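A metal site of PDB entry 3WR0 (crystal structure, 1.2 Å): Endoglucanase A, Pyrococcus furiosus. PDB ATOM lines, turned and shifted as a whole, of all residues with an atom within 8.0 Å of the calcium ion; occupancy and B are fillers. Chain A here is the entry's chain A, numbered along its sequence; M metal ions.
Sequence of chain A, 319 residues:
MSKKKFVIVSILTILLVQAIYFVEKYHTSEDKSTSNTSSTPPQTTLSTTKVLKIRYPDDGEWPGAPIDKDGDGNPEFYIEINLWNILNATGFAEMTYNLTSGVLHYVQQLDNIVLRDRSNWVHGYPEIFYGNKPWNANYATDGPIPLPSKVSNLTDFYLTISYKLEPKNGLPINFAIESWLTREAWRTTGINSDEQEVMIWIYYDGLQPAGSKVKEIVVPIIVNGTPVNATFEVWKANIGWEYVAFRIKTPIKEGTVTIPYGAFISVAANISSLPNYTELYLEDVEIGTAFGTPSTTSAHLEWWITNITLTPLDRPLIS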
ATOM      1  N   ILE A  67      12.759 -22.908  15.007  1.00  0.00           N
ATOM      2  CA  ILE A  67      12.189 -21.555  15.161  1.00  0.00           C
ATOM      3  C   ILE A  67      12.686 -21.076  16.524  1.00  0.00           C
ATOM      4  O   ILE A  67      12.305 -21.674  17.568  1.00  0.00           O
ATOM      5  CB  ILE A  67      10.636 -21.632  15.124  1.00  0.00           C
ATOM      6  CG1 ILE A  67      10.211 -21.962  13.686  1.00  0.00           C
ATOM      7  CG2 ILE A  67      10.066 -20.298  15.563  1.00  0.00           C
ATOM      8  CD1 ILE A  67       8.743 -22.291  13.590  1.00  0.00           C
ATOM      9  N   ASP A  68      13.485 -20.020  16.523  1.00  0.00           N
ATOM     10  CA  ASP A  68      14.072 -19.529  17.773  1.00  0.00           C
ATOM     11  C   ASP A  68      14.024 -18.007  17.694  1.00  0.00           C
ATOM     12  O   ASP A  68      15.018 -17.321  17.405  1.00  0.00           O
ATOM     13  CB  ASP A  68      15.553 -20.012  17.823  1.00  0.00           C
ATOM     14  CG  ASP A  68      16.273 -19.631  19.138  1.00  0.00           C
ATOM     15  OD1 ASP A  68      15.615 -19.231  20.069  1.00  0.00           O
ATOM     16  OD2 ASP A  68      17.520 -19.755  19.096  1.00  0.00           O
ATOM     17  N   LYS A  69      12.868 -17.458  18.026  1.00  0.00           N
ATOM     18  CA  LYS A  69      12.603 -16.039  17.741  1.00  0.00           C
ATOM     19  C   LYS A  69      13.468 -15.120  18.605  1.00  0.00           C
ATOM     20  O   LYS A  69      13.777 -13.996  18.190  1.00  0.00           O
ATOM     21  CB  LYS A  69      11.144 -15.745  18.067  1.00  0.00           C
ATOM     22  CG  LYS A  69      10.822 -14.268  17.845  1.00  0.00           C
ATOM     23  CD  LYS A  69       9.342 -14.072  17.762  1.00  0.00           C
ATOM     24  CE  LYS A  69       9.056 -12.595  17.521  1.00  0.00           C
ATOM     25  NZ  LYS A  69       9.957 -11.946  16.510  1.00  0.00           N
ATOM     26  N   ASP A  70      13.775 -15.542  19.859  1.00  0.00           N
ATOM     27  CA  ASP A  70      14.634 -14.722  20.727  1.00  0.00           C
ATOM     28  C   ASP A  70      16.119 -15.058  20.533  1.00  0.00           C
ATOM     29  O   ASP A  70      16.946 -14.436  21.203  1.00  0.00           O
ATOM     30  CB  ASP A  70      14.168 -14.830  22.194  1.00  0.00           C
ATOM     31  CG  ASP A  70      14.318 -16.174  22.797  1.00  0.00           C
ATOM     32  OD1 ASP A  70      14.431 -17.174  22.049  1.00  0.00           O
ATOM     33  OD2 ASP A  70      14.242 -16.358  24.026  1.00  0.00           O
ATOM     34  N   GLY A  71      16.460 -15.954  19.578  1.00  0.00           N
ATOM     35  CA  GLY A  71      17.865 -16.244  19.297  1.00  0.00           C
ATOM     36  C   GLY A  71      18.580 -16.783  20.531  1.00  0.00           C
ATOM     37  O   GLY A  71      19.797 -16.554  20.634  1.00  0.00           O
ATOM     38  N   ASP A  72      17.903 -17.477  21.451  1.00  0.00           N
ATOM     39  CA  ASP A  72      18.570 -17.959  22.661  1.00  0.00           C
ATOM     40  C   ASP A  72      19.129 -19.335  22.555  1.00  0.00           C
ATOM     41  O   ASP A  72      19.682 -19.821  23.572  1.00  0.00           O
ATOM     42  CB  ASP A  72      17.733 -17.724  23.876  1.00  0.00           C
ATOM     43  CG  ASP A  72      16.633 -18.751  24.116  1.00  0.00           C
ATOM     44  OD1 ASP A  72      16.313 -19.478  23.136  1.00  0.00           O
ATOM     45  OD2 ASP A  72      16.102 -18.829  25.254  1.00  0.00           O
ATOM     46  N   GLY A  73      19.066 -19.970  21.431  1.00  0.00           N
ATOM     47  CA  GLY A  73      19.636 -21.323  21.277  1.00  0.00           C
ATOM     48  C   GLY A  73      18.725 -22.437  21.705  1.00  0.00           C
ATOM     49  O   GLY A  73      19.125 -23.634  21.659  1.00  0.00           O
ATOM     50  N   ASN A  74      17.498 -22.075  22.189  1.00  0.00           N
ATOM     51  CA  ASN A  74      16.508 -23.100  22.556  1.00  0.00           C
ATOM     52  C   ASN A  74      15.298 -22.847  21.668  1.00  0.00           C
ATOM     53  O   ASN A  74      14.632 -21.795  21.859  1.00  0.00           O
ATOM     54  CB  ASN A  74      16.139 -22.979  24.005  1.00  0.00           C
ATOM     55  CG  ASN A  74      15.310 -24.172  24.528  1.00  0.00           C
ATOM     56  OD1 ASN A  74      15.093 -25.112  23.762  1.00  0.00           O
ATOM     57  ND2 ASN A  74      14.912 -24.097  25.792  1.00  0.00           N
ATOM     58  N   PRO A  75      15.013 -23.674  20.704  1.00  0.00           N
ATOM     59  CA  PRO A  75      13.888 -23.349  19.795  1.00  0.00           C
ATOM     60  C   PRO A  75      12.572 -23.424  20.545  1.00  0.00           C
ATOM     61  O   PRO A  75      12.359 -24.269  21.445  1.00  0.00           O
ATOM     62  CB  PRO A  75      13.981 -24.467  18.742  1.00  0.00           C
ATOM     63  CG  PRO A  75      15.414 -24.971  18.803  1.00  0.00           C
ATOM     64  CD  PRO A  75      15.718 -24.887  20.308  1.00  0.00           C
ATOM     65  N   GLU A  76      11.648 -22.528  20.161  1.00  0.00           N
ATOM     66  CA  GLU A  76      10.250 -22.641  20.626  1.00  0.00           C
ATOM     67  C   GLU A  76       9.498 -23.738  19.897  1.00  0.00           C
ATOM     68  O   GLU A  76       8.597 -24.365  20.478  1.00  0.00           O
ATOM     69  CB  GLU A  76       9.472 -21.332  20.374  1.00  0.00           C
ATOM     70  CG  GLU A  76      10.111 -20.192  21.156  1.00  0.00           C
ATOM     71  CD  GLU A  76      11.205 -19.496  20.266  1.00  0.00           C
ATOM     72  OE1 GLU A  76      10.937 -19.057  19.102  1.00  0.00           O
ATOM     73  OE2 GLU A  76      12.370 -19.312  20.745  1.00  0.00           O
ATOM     74  N   PHE A  77       9.862 -23.987  18.588  1.00  0.00           N
ATOM     75  CA  PHE A  77       9.251 -25.049  17.801  1.00  0.00           C
ATOM     76  C   PHE A  77      10.327 -25.458  16.843  1.00  0.00           C
ATOM     77  O   PHE A  77      11.333 -24.772  16.625  1.00  0.00           O
ATOM     78  CB  PHE A  77       8.008 -24.544  17.002  1.00  0.00           C
ATOM     79  CG  PHE A  77       6.882 -24.174  17.864  1.00  0.00           C
ATOM     80  CD1 PHE A  77       6.052 -25.149  18.385  1.00  0.00           C
ATOM     81  CD2 PHE A  77       6.641 -22.859  18.243  1.00  0.00           C
ATOM     82  CE1 PHE A  77       5.002 -24.893  19.269  1.00  0.00           C
ATOM     83  CE2 PHE A  77       5.623 -22.525  19.098  1.00  0.00           C
ATOM     84  CZ  PHE A  77       4.800 -23.551  19.614  1.00  0.00           C
ATOM     85  N   THR A 141      12.431 -26.773  23.140  1.00  0.00           N
ATOM     86  CA  THR A 141      12.029 -26.835  24.524  1.00  0.00           C
ATOM     87  C   THR A 141      11.801 -25.488  25.126  1.00  0.00           C
ATOM     88  O   THR A 141      11.639 -25.386  26.352  1.00  0.00           O
ATOM     89  CB  THR A 141      12.963 -27.710  25.371  1.00  0.00           C
ATOM     90  OG1 THR A 141      14.220 -27.074  25.510  1.00  0.00           O
ATOM     91  CG2 THR A 141      13.042 -29.120  24.866  1.00  0.00           C
ATOM     92  N   ASP A 142      11.693 -24.406  24.327  1.00  0.00           N
ATOM     93  CA  ASP A 142      11.462 -23.055  24.845  1.00  0.00           C
ATOM     94  C   ASP A 142       9.944 -22.852  24.894  1.00  0.00           C
ATOM     95  O   ASP A 142       9.356 -22.337  23.917  1.00  0.00           O
ATOM     96  CB  ASP A 142      12.210 -22.066  23.996  1.00  0.00           C
ATOM     97  CG  ASP A 142      12.227 -20.639  24.560  1.00  0.00           C
ATOM     98  OD1 ASP A 142      11.515 -20.358  25.544  1.00  0.00           O
ATOM     99  OD2 ASP A 142      12.953 -19.818  23.942  1.00  0.00           O
ATOM    100  N   GLY A 143       9.277 -23.314  25.926  1.00  0.00           N
ATOM    101  CA  GLY A 143       7.835 -23.215  26.054  1.00  0.00           C
ATOM    102  C   GLY A 143       7.415 -23.529  27.477  1.00  0.00           C
ATOM    103  O   GLY A 143       8.255 -24.008  28.303  1.00  0.00           O
HETATM  104 CA    CA M   1      14.254 -19.509  21.999  1.00  0.00          CA
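N of Glu 76 sits at hydrogen-bond distance from O of Ile 67 (2.8 Å). OD1 of Asn 74 sits at hydrogen-bond distance from OG1 of Thr 141 (2.8 Å). The side-chain carboxylate (OE1) of Glu 76 lies within hydrogen-bond range of the backbone NH (N) of Lys 69, at 2.7 Å. The side-chain carboxylate (OD1) of Asp 68 lies close to the backbone NH (N) of Gly 71 (3.4 Å). The side-chain carboxylate (OD2) of Asp 68 sits at hydrogen-bond distance from the backbone NH (N) of Gly 73 (2.8 Å). The backbone NH (N) of Asp 142 lies within hydrogen-bond range of the backbone carbonyl oxygen (O) of Pro 75.
Within 4 Å of the calcium ion: Asp 68, Asp 70, Asp 72, Asn 74, Glu 76 and Asp 142. The nearest printed residue that does not touch the calcium ion is Pro 75 (4.4 Å).
The calcium ion is bound by the side-chain carboxylate of Glu 76 (2.3 Å), the backbone carbonyl oxygen of Asn 74 (2.3 Å), the side-chain carboxylate of Asp 70 (2.3 Å), the side-chain carboxylate of Asp 72 (2.4 Å), the side-chain carboxylate of Asp 142 (2.4 Å) and the side-chain carboxylate of Asp 68 (2.4 Å). The calcium ion has six donor atoms within binding distance.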
